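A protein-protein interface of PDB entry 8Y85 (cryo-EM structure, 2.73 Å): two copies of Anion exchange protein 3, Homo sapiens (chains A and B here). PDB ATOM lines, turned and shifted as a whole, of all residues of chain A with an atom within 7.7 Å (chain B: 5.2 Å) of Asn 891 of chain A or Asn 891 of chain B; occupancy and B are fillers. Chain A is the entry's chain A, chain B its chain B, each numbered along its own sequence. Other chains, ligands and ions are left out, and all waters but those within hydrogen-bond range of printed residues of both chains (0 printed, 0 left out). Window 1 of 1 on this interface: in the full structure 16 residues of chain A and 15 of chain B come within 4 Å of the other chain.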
ATOM      1  N   HIS A 850      23.279  13.946   8.937  1.00  0.00           N
ATOM      2  CA  HIS A 850      23.233  15.014   7.938  1.00  0.00           C
ATOM      3  C   HIS A 850      24.445  14.944   7.013  1.00  0.00           C
ATOM      4  O   HIS A 850      25.362  15.769   7.106  1.00  0.00           O
ATOM      5  CB  HIS A 850      23.160  16.369   8.634  1.00  0.00           C
ATOM      6  CG  HIS A 850      21.953  16.526   9.501  1.00  0.00           C
ATOM      7  ND1 HIS A 850      20.703  16.828   9.004  1.00  0.00           N
ATOM      8  CD2 HIS A 850      21.808  16.418  10.841  1.00  0.00           C
ATOM      9  CE1 HIS A 850      19.842  16.900  10.003  1.00  0.00           C
ATOM     10  NE2 HIS A 850      20.488  16.656  11.128  1.00  0.00           N
ATOM     11  N   PRO A 851      24.463  13.993   6.082  1.00  0.00           N
ATOM     12  CA  PRO A 851      25.620  13.854   5.190  1.00  0.00           C
ATOM     13  C   PRO A 851      25.702  14.985   4.174  1.00  0.00           C
ATOM     14  O   PRO A 851      24.723  15.674   3.880  1.00  0.00           O
ATOM     15  CB  PRO A 851      25.373  12.508   4.499  1.00  0.00           C
ATOM     16  CG  PRO A 851      23.901  12.349   4.526  1.00  0.00           C
ATOM     17  CD  PRO A 851      23.412  13.009   5.783  1.00  0.00           C
ATOM     18  N   LEU A 852      26.906  15.172   3.636  1.00  0.00           N
ATOM     19  CA  LEU A 852      27.148  16.180   2.609  1.00  0.00           C
ATOM     20  C   LEU A 852      26.714  15.619   1.260  1.00  0.00           C
ATOM     21  O   LEU A 852      27.313  14.663   0.756  1.00  0.00           O
ATOM     22  CB  LEU A 852      28.619  16.585   2.591  1.00  0.00           C
ATOM     23  CG  LEU A 852      29.202  17.201   3.865  1.00  0.00           C
ATOM     24  CD1 LEU A 852      30.560  17.812   3.581  1.00  0.00           C
ATOM     25  CD2 LEU A 852      28.265  18.241   4.451  1.00  0.00           C
ATOM     26  N   LEU A 853      25.674  16.209   0.672  1.00  0.00           N
ATOM     27  CA  LEU A 853      25.109  15.692  -0.563  1.00  0.00           C
ATOM     28  C   LEU A 853      25.240  16.711  -1.689  1.00  0.00           C
ATOM     29  O   LEU A 853      25.234  17.921  -1.441  1.00  0.00           O
ATOM     30  CB  LEU A 853      23.630  15.324  -0.386  1.00  0.00           C
ATOM     31  CG  LEU A 853      23.325  14.219   0.625  1.00  0.00           C
ATOM     32  CD1 LEU A 853      21.830  14.090   0.838  1.00  0.00           C
ATOM     33  CD2 LEU A 853      23.922  12.898   0.172  1.00  0.00           C
ATOM     34  N   PRO A 854      25.380  16.251  -2.935  1.00  0.00           N
ATOM     35  CA  PRO A 854      25.449  17.202  -4.055  1.00  0.00           C
ATOM     36  C   PRO A 854      24.171  17.995  -4.245  1.00  0.00           C
ATOM     37  O   PRO A 854      24.224  19.197  -4.536  1.00  0.00           O
ATOM     38  CB  PRO A 854      25.735  16.297  -5.263  1.00  0.00           C
ATOM     39  CG  PRO A 854      26.290  15.038  -4.684  1.00  0.00           C
ATOM     40  CD  PRO A 854      25.587  14.862  -3.376  1.00  0.00           C
ATOM     41  N   PHE A 855      23.019  17.352  -4.088  1.00  0.00           N
ATOM     42  CA  PHE A 855      21.725  17.985  -4.289  1.00  0.00           C
ATOM     43  C   PHE A 855      20.860  17.783  -3.056  1.00  0.00           C
ATOM     44  O   PHE A 855      20.820  16.688  -2.489  1.00  0.00           O
ATOM     45  CB  PHE A 855      21.014  17.422  -5.529  1.00  0.00           C
ATOM     46  CG  PHE A 855      21.475  18.031  -6.820  1.00  0.00           C
ATOM     47  CD1 PHE A 855      21.159  19.342  -7.129  1.00  0.00           C
ATOM     48  CD2 PHE A 855      22.233  17.300  -7.718  1.00  0.00           C
ATOM     49  CE1 PHE A 855      21.584  19.912  -8.312  1.00  0.00           C
ATOM     50  CE2 PHE A 855      22.662  17.866  -8.903  1.00  0.00           C
ATOM     51  CZ  PHE A 855      22.336  19.174  -9.200  1.00  0.00           C
ATOM     52  N   TYR A 856      20.172  18.843  -2.648  1.00  0.00           N
ATOM     53  CA  TYR A 856      19.280  18.807  -1.490  1.00  0.00           C
ATOM     54  C   TYR A 856      17.877  19.188  -1.936  1.00  0.00           C
ATOM     55  O   TYR A 856      17.561  20.386  -2.043  1.00  0.00           O
ATOM     56  CB  TYR A 856      19.777  19.747  -0.393  1.00  0.00           C
ATOM     57  CG  TYR A 856      20.996  19.227   0.328  1.00  0.00           C
ATOM     58  CD1 TYR A 856      20.906  18.145   1.191  1.00  0.00           C
ATOM     59  CD2 TYR A 856      22.242  19.805   0.133  1.00  0.00           C
ATOM     60  CE1 TYR A 856      22.018  17.661   1.847  1.00  0.00           C
ATOM     61  CE2 TYR A 856      23.361  19.327   0.785  1.00  0.00           C
ATOM     62  CZ  TYR A 856      23.243  18.255   1.641  1.00  0.00           C
ATOM     63  OH  TYR A 856      24.355  17.777   2.293  1.00  0.00           O
ATOM     64  N   ASN A 888      18.888  15.001   6.756  1.00  0.00           N
ATOM     65  CA  ASN A 888      19.442  15.352   5.449  1.00  0.00           C
ATOM     66  C   ASN A 888      19.388  16.861   5.210  1.00  0.00           C
ATOM     67  O   ASN A 888      18.887  17.336   4.189  1.00  0.00           O
ATOM     68  CB  ASN A 888      18.725  14.593   4.329  1.00  0.00           C
ATOM     69  CG  ASN A 888      19.057  13.116   4.316  1.00  0.00           C
ATOM     70  OD1 ASN A 888      20.217  12.728   4.443  1.00  0.00           O
ATOM     71  ND2 ASN A 888      18.037  12.281   4.164  1.00  0.00           N
ATOM     72  N   GLN A 889      19.915  17.620   6.174  1.00  0.00           N
ATOM     73  CA  GLN A 889      19.958  19.069   6.077  1.00  0.00           C
ATOM     74  C   GLN A 889      21.347  19.540   5.661  1.00  0.00           C
ATOM     75  O   GLN A 889      22.353  18.929   6.031  1.00  0.00           O
ATOM     76  CB  GLN A 889      19.585  19.712   7.416  1.00  0.00           C
ATOM     77  CG  GLN A 889      18.209  19.324   7.921  1.00  0.00           C
ATOM     78  CD  GLN A 889      17.093  20.080   7.231  1.00  0.00           C
ATOM     79  OE1 GLN A 889      17.199  21.281   6.993  1.00  0.00           O
ATOM     80  NE2 GLN A 889      16.016  19.378   6.901  1.00  0.00           N
ATOM     81  N   PRO A 890      21.433  20.614   4.880  1.00  0.00           N
ATOM     82  CA  PRO A 890      22.739  21.162   4.505  1.00  0.00           C
ATOM     83  C   PRO A 890      23.298  22.112   5.553  1.00  0.00           C
ATOM     84  O   PRO A 890      22.571  22.725   6.337  1.00  0.00           O
ATOM     85  CB  PRO A 890      22.431  21.914   3.203  1.00  0.00           C
ATOM     86  CG  PRO A 890      21.016  22.326   3.346  1.00  0.00           C
ATOM     87  CD  PRO A 890      20.328  21.254   4.144  1.00  0.00           C
ATOM     88  N   ASN A 891      24.628  22.212   5.555  1.00  0.00           N
ATOM     89  CA  ASN A 891      25.385  23.150   6.379  1.00  0.00           C
ATOM     90  C   ASN A 891      25.240  22.889   7.874  1.00  0.00           C
ATOM     91  O   ASN A 891      25.485  23.787   8.683  1.00  0.00           O
ATOM     92  CB  ASN A 891      24.991  24.598   6.067  1.00  0.00           C
ATOM     93  CG  ASN A 891      24.989  24.892   4.586  1.00  0.00           C
ATOM     94  OD1 ASN A 891      25.881  24.466   3.858  1.00  0.00           O
ATOM     95  ND2 ASN A 891      23.978  25.616   4.129  1.00  0.00           N
ATOM     96  N   THR A 892      24.851  21.676   8.271  1.00  0.00           N
ATOM     97  CA  THR A 892      24.637  21.369   9.682  1.00  0.00           C
ATOM     98  C   THR A 892      25.868  20.743  10.328  1.00  0.00           C
ATOM     99  O   THR A 892      26.342  21.218  11.365  1.00  0.00           O
ATOM    100  CB  THR A 892      23.429  20.438   9.842  1.00  0.00           C
ATOM    101  OG1 THR A 892      22.242  21.113   9.408  1.00  0.00           O
ATOM    102  CG2 THR A 892      23.261  20.010  11.293  1.00  0.00           C
ATOM    103  N   ALA A 893      26.394  19.680   9.719  1.00  0.00           N
ATOM    104  CA  ALA A 893      27.522  18.968  10.304  1.00  0.00           C
ATOM    105  C   ALA A 893      28.774  19.835  10.359  1.00  0.00           C
ATOM    106  O   ALA A 893      29.485  19.846  11.373  1.00  0.00           O
ATOM    107  CB  ALA A 893      27.781  17.693   9.509  1.00  0.00           C
ATOM    108  N   LEU A 894      29.065  20.563   9.280  1.00  0.00           N
ATOM    109  CA  LEU A 894      30.253  21.412   9.258  1.00  0.00           C
ATOM    110  C   LEU A 894      30.138  22.545  10.268  1.00  0.00           C
ATOM    111  O   LEU A 894      31.123  22.898  10.928  1.00  0.00           O
ATOM    112  CB  LEU A 894      30.479  21.958   7.850  1.00  0.00           C
ATOM    113  CG  LEU A 894      30.881  20.935   6.782  1.00  0.00           C
ATOM    114  CD1 LEU A 894      30.851  21.561   5.404  1.00  0.00           C
ATOM    115  CD2 LEU A 894      32.246  20.343   7.070  1.00  0.00           C
ATOM    116  N   LEU A 895      28.945  23.121  10.406  1.00  0.00           N
ATOM    117  CA  LEU A 895      28.735  24.159  11.409  1.00  0.00           C
ATOM    118  C   LEU A 895      28.903  23.607  12.820  1.00  0.00           C
ATOM    119  O   LEU A 895      29.450  24.286  13.697  1.00  0.00           O
ATOM    120  CB  LEU A 895      27.354  24.786  11.232  1.00  0.00           C
ATOM    121  CG  LEU A 895      27.066  26.040  12.057  1.00  0.00           C
ATOM    122  CD1 LEU A 895      28.011  27.162  11.678  1.00  0.00           C
ATOM    123  CD2 LEU A 895      25.625  26.474  11.884  1.00  0.00           C
ATOM    124  N   SER A 896      28.432  22.381  13.063  1.00  0.00           N
ATOM    125  CA  SER A 896      28.631  21.761  14.370  1.00  0.00           C
ATOM    126  C   SER A 896      30.112  21.558  14.663  1.00  0.00           C
ATOM    127  O   SER A 896      30.576  21.812  15.784  1.00  0.00           O
ATOM    128  CB  SER A 896      27.886  20.429  14.439  1.00  0.00           C
ATOM    129  OG  SER A 896      26.500  20.607  14.222  1.00  0.00           O
ATOM    130  N   ILE A 946      23.602  33.423  13.154  1.00  0.00           N
ATOM    131  CA  ILE A 946      23.243  32.718  11.928  1.00  0.00           C
ATOM    132  C   ILE A 946      21.836  32.157  12.098  1.00  0.00           C
ATOM    133  O   ILE A 946      21.641  31.170  12.810  1.00  0.00           O
ATOM    134  CB  ILE A 946      24.240  31.598  11.613  1.00  0.00           C
ATOM    135  CG1 ILE A 946      25.672  32.054  11.886  1.00  0.00           C
ATOM    136  CG2 ILE A 946      24.072  31.116  10.184  1.00  0.00           C
ATOM    137  CD1 ILE A 946      26.697  30.963  11.678  1.00  0.00           C
ATOM    138  N   ASP A 948      19.761  30.818   9.430  1.00  0.00           N
ATOM    139  CA  ASP A 948      19.283  30.112   8.245  1.00  0.00           C
ATOM    140  C   ASP A 948      19.400  28.602   8.361  1.00  0.00           C
ATOM    141  O   ASP A 948      18.684  27.891   7.647  1.00  0.00           O
ATOM    142  CB  ASP A 948      20.033  30.570   6.988  1.00  0.00           C
ATOM    143  CG  ASP A 948      20.020  32.076   6.811  1.00  0.00           C
ATOM    144  OD1 ASP A 948      20.868  32.757   7.425  1.00  0.00           O
ATOM    145  OD2 ASP A 948      19.155  32.578   6.062  1.00  0.00           O
ATOM    146  N   THR A 949      20.267  28.086   9.228  1.00  0.00           N
ATOM    147  CA  THR A 949      20.637  26.682   9.277  1.00  0.00           C
ATOM    148  C   THR A 949      20.066  26.029  10.529  1.00  0.00           C
ATOM    149  O   THR A 949      19.849  26.687  11.551  1.00  0.00           O
ATOM    150  CB  THR A 949      22.163  26.528   9.259  1.00  0.00           C
ATOM    151  OG1 THR A 949      22.724  27.465   8.334  1.00  0.00           O
ATOM    152  CG2 THR A 949      22.565  25.132   8.835  1.00  0.00           C
ATOM    153  N   TYR A 950      19.823  24.726  10.438  1.00  0.00           N
ATOM    154  CA  TYR A 950      19.315  23.949  11.557  1.00  0.00           C
ATOM    155  C   TYR A 950      20.469  23.368  12.363  1.00  0.00           C
ATOM    156  O   TYR A 950      21.374  22.741  11.804  1.00  0.00           O
ATOM    157  CB  TYR A 950      18.408  22.821  11.063  1.00  0.00           C
ATOM    158  CG  TYR A 950      18.140  21.762  12.106  1.00  0.00           C
ATOM    159  CD1 TYR A 950      17.282  22.008  13.168  1.00  0.00           C
ATOM    160  CD2 TYR A 950      18.754  20.520  12.036  1.00  0.00           C
ATOM    161  CE1 TYR A 950      17.038  21.045  14.124  1.00  0.00           C
ATOM    162  CE2 TYR A 950      18.518  19.553  12.988  1.00  0.00           C
ATOM    163  CZ  TYR A 950      17.658  19.820  14.029  1.00  0.00           C
ATOM    164  OH  TYR A 950      17.417  18.859  14.982  1.00  0.00           O
ATOM    165  N   THR A 951      20.432  23.586  13.675  1.00  0.00           N
ATOM    166  CA  THR A 951      21.335  22.943  14.616  1.00  0.00           C
ATOM    167  C   THR A 951      20.512  22.347  15.749  1.00  0.00           C
ATOM    168  O   THR A 951      19.481  22.898  16.140  1.00  0.00           O
ATOM    169  CB  THR A 951      22.372  23.927  15.184  1.00  0.00           C
ATOM    170  OG1 THR A 951      21.735  25.168  15.506  1.00  0.00           O
ATOM    171  CG2 THR A 951      23.485  24.179  14.177  1.00  0.00           C
ATOM    172  N   LEU B 852      24.740  30.860   2.813  1.00  0.00           N
ATOM    173  CA  LEU B 852      24.043  29.754   3.463  1.00  0.00           C
ATOM    174  C   LEU B 852      22.542  29.968   3.319  1.00  0.00           C
ATOM    175  O   LEU B 852      21.989  30.924   3.873  1.00  0.00           O
ATOM    176  CB  LEU B 852      24.449  29.656   4.930  1.00  0.00           C
ATOM    177  CG  LEU B 852      25.929  29.431   5.248  1.00  0.00           C
ATOM    178  CD1 LEU B 852      26.109  29.068   6.709  1.00  0.00           C
ATOM    179  CD2 LEU B 852      26.524  28.353   4.358  1.00  0.00           C
ATOM    180  N   LEU B 853      21.877  29.081   2.579  1.00  0.00           N
ATOM    181  CA  LEU B 853      20.461  29.249   2.296  1.00  0.00           C
ATOM    182  C   LEU B 853      19.648  28.105   2.889  1.00  0.00           C
ATOM    183  O   LEU B 853      20.131  26.972   2.976  1.00  0.00           O
ATOM    184  CB  LEU B 853      20.202  29.322   0.785  1.00  0.00           C
ATOM    185  CG  LEU B 853      20.854  30.486   0.041  1.00  0.00           C
ATOM    186  CD1 LEU B 853      20.679  30.326  -1.457  1.00  0.00           C
ATOM    187  CD2 LEU B 853      20.281  31.811   0.512  1.00  0.00           C
ATOM    188  N   TYR B 856      18.063  24.745  -1.316  1.00  0.00           N
ATOM    189  CA  TYR B 856      18.966  24.742  -2.466  1.00  0.00           C
ATOM    190  C   TYR B 856      18.310  23.947  -3.585  1.00  0.00           C
ATOM    191  O   TYR B 856      18.528  22.736  -3.713  1.00  0.00           O
ATOM    192  CB  TYR B 856      20.328  24.161  -2.096  1.00  0.00           C
ATOM    193  CG  TYR B 856      21.159  25.084  -1.238  1.00  0.00           C
ATOM    194  CD1 TYR B 856      21.692  26.253  -1.758  1.00  0.00           C
ATOM    195  CD2 TYR B 856      21.399  24.792   0.098  1.00  0.00           C
ATOM    196  CE1 TYR B 856      22.447  27.102  -0.977  1.00  0.00           C
ATOM    197  CE2 TYR B 856      22.153  25.635   0.886  1.00  0.00           C
ATOM    198  CZ  TYR B 856      22.675  26.788   0.344  1.00  0.00           C
ATOM    199  OH  TYR B 856      23.427  27.631   1.126  1.00  0.00           O
ATOM    200  N   GLN B 889      26.101  27.360  -4.201  1.00  0.00           N
ATOM    201  CA  GLN B 889      26.333  25.963  -3.869  1.00  0.00           C
ATOM    202  C   GLN B 889      26.333  25.765  -2.356  1.00  0.00           C
ATOM    203  O   GLN B 889      26.742  26.657  -1.607  1.00  0.00           O
ATOM    204  CB  GLN B 889      27.666  25.493  -4.442  1.00  0.00           C
ATOM    205  CG  GLN B 889      27.800  25.684  -5.940  1.00  0.00           C
ATOM    206  CD  GLN B 889      27.003  24.672  -6.739  1.00  0.00           C
ATOM    207  OE1 GLN B 889      27.438  23.538  -6.928  1.00  0.00           O
ATOM    208  NE2 GLN B 889      25.836  25.079  -7.220  1.00  0.00           N
ATOM    209  N   PRO B 890      25.868  24.613  -1.882  1.00  0.00           N
ATOM    210  CA  PRO B 890      25.928  24.316  -0.449  1.00  0.00           C
ATOM    211  C   PRO B 890      27.258  23.704  -0.036  1.00  0.00           C
ATOM    212  O   PRO B 890      27.964  23.076  -0.827  1.00  0.00           O
ATOM    213  CB  PRO B 890      24.786  23.307  -0.262  1.00  0.00           C
ATOM    214  CG  PRO B 890      24.699  22.612  -1.567  1.00  0.00           C
ATOM    215  CD  PRO B 890      25.069  23.619  -2.622  1.00  0.00           C
ATOM    216  N   ASN B 891      27.592  23.915   1.238  1.00  0.00           N
ATOM    217  CA  ASN B 891      28.756  23.326   1.894  1.00  0.00           C
ATOM    218  C   ASN B 891      30.082  23.798   1.305  1.00  0.00           C
ATOM    219  O   ASN B 891      31.106  23.134   1.485  1.00  0.00           O
ATOM    220  CB  ASN B 891      28.691  21.795   1.862  1.00  0.00           C
ATOM    221  CG  ASN B 891      27.356  21.263   2.328  1.00  0.00           C
ATOM    222  OD1 ASN B 891      26.791  21.748   3.305  1.00  0.00           O
ATOM    223  ND2 ASN B 891      26.839  20.266   1.624  1.00  0.00           N
ATOM    224  N   THR B 892      30.096  24.933   0.607  1.00  0.00           N
ATOM    225  CA  THR B 892      31.317  25.432  -0.019  1.00  0.00           C
ATOM    226  C   THR B 892      32.061  26.419   0.877  1.00  0.00           C
ATOM    227  O   THR B 892      33.262  26.262   1.117  1.00  0.00           O
ATOM    228  CB  THR B 892      30.990  26.086  -1.367  1.00  0.00           C
ATOM    229  OG1 THR B 892      30.464  25.100  -2.263  1.00  0.00           O
ATOM    230  CG2 THR B 892      32.234  26.710  -1.984  1.00  0.00           C
ATOM    231  N   ALA B 893      31.354  27.432   1.380  1.00  0.00           N
ATOM    232  CA  ALA B 893      31.994  28.470   2.180  1.00  0.00           C
ATOM    233  C   ALA B 893      32.568  27.905   3.474  1.00  0.00           C
ATOM    234  O   ALA B 893      33.711  28.206   3.845  1.00  0.00           O
ATOM    235  CB  ALA B 893      30.990  29.581   2.477  1.00  0.00           C
ATOM    236  N   LEU B 894      31.785  27.090   4.182  1.00  0.00           N
ATOM    237  CA  LEU B 894      32.247  26.540   5.452  1.00  0.00           C
ATOM    238  C   LEU B 894      33.428  25.603   5.248  1.00  0.00           C
ATOM    239  O   LEU B 894      34.367  25.592   6.052  1.00  0.00           O
ATOM    240  CB  LEU B 894      31.098  25.827   6.162  1.00  0.00           C
ATOM    241  CG  LEU B 894      29.955  26.721   6.654  1.00  0.00           C
ATOM    242  CD1 LEU B 894      28.777  25.884   7.110  1.00  0.00           C
ATOM    243  CD2 LEU B 894      30.411  27.647   7.763  1.00  0.00           C
ATOM    244  N   LEU B 895      33.402  24.812   4.175  1.00  0.00           N
ATOM    245  CA  LEU B 895      34.532  23.942   3.868  1.00  0.00           C
ATOM    246  C   LEU B 895      35.782  24.752   3.543  1.00  0.00           C
ATOM    247  O   LEU B 895      36.891  24.374   3.939  1.00  0.00           O
ATOM    248  CB  LEU B 895      34.174  23.011   2.712  1.00  0.00           C
ATOM    249  CG  LEU B 895      35.169  21.889   2.415  1.00  0.00           C
ATOM    250  CD1 LEU B 895      35.292  20.952   3.600  1.00  0.00           C
ATOM    251  CD2 LEU B 895      34.761  21.127   1.171  1.00  0.00           C
ATOM    252  N   THR B 949      31.391  17.933  -2.873  1.00  0.00           N
ATOM    253  CA  THR B 949      31.187  19.368  -2.760  1.00  0.00           C
ATOM    254  C   THR B 949      32.107  20.104  -3.725  1.00  0.00           C
ATOM    255  O   THR B 949      33.219  19.655  -4.016  1.00  0.00           O
ATOM    256  CB  THR B 949      31.451  19.838  -1.324  1.00  0.00           C
ATOM    257  OG1 THR B 949      30.805  18.946  -0.408  1.00  0.00           O
ATOM    258  CG2 THR B 949      30.916  21.234  -1.101  1.00  0.00           C
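OD1 of Asn 891 of chain B lies close to OD1 of Asn 891 of chain A (2.9 Å).
O of Tyr 856 of chain A lies close to O of Tyr 856 of chain B (3.0 Å).
O of Pro 851 of chain A is in hydrogen-bond range of OH of Tyr 856 of chain A (2.7 Å).
OH of Tyr 856 of chain A lies within hydrogen-bond range of N of Leu 853 of chain A.
OH of Tyr 856 of chain B sits at hydrogen-bond distance from N of Leu 853 of chain B, 2.6 Å away.
Among the printed residues, pairs that only touch across the chains: Leu 852 of chain A with Asn 891 of chain B, Tyr 856 of chain A with Asn 891 of chain B, Asn 891 of chain A with Leu 852 of chain B, Asn 891 of chain A with Tyr 856 of chain B and Asp 948 of chain A with Leu 852 of chain B.
Of the printed residues of chain B, Tyr 856 of chain A touches Tyr 856 and Asn 891.
Of the printed residues of chain A, Leu 852 of chain B touches Asn 891 (3.7 Å) and Asp 948 (3.7 Å).
Asn 891 of chain B touches three residues of chain A.
The nearest printed residue of chain B that does not touch Leu 852 of chain A is Thr 949 of chain B (4.2 Å).
Hydrophobic or aromatic side chains of chain B that line the printed part of chain A: Leu 852 and Tyr 856.
Along chain A the printed residues that touch a printed residue of chain B span positions 852 to 948.
Among the printed residues, 7 pairs touch across the chains.
Among the printed residues, no Asp or Glu carboxylate lies within 4 Å of a Lys or Arg side-chain nitrogen of the other chain.
Leu 852 of chain A touches Asn 891 of chain B, and with the chains exchanged Asn 891 of chain A touches Leu 852 of chain B.
Tyr 856 of chain B touches its own counterpart, Tyr 856 of chain A.
Tyr 856 of chain A touches Asn 891 of chain B, and with the chains exchanged Asn 891 of chain A touches Tyr 856 of chain B.
Asn 891 of chain B touches its own counterpart, Asn 891 of chain A.
11 positions are printed for both chains.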
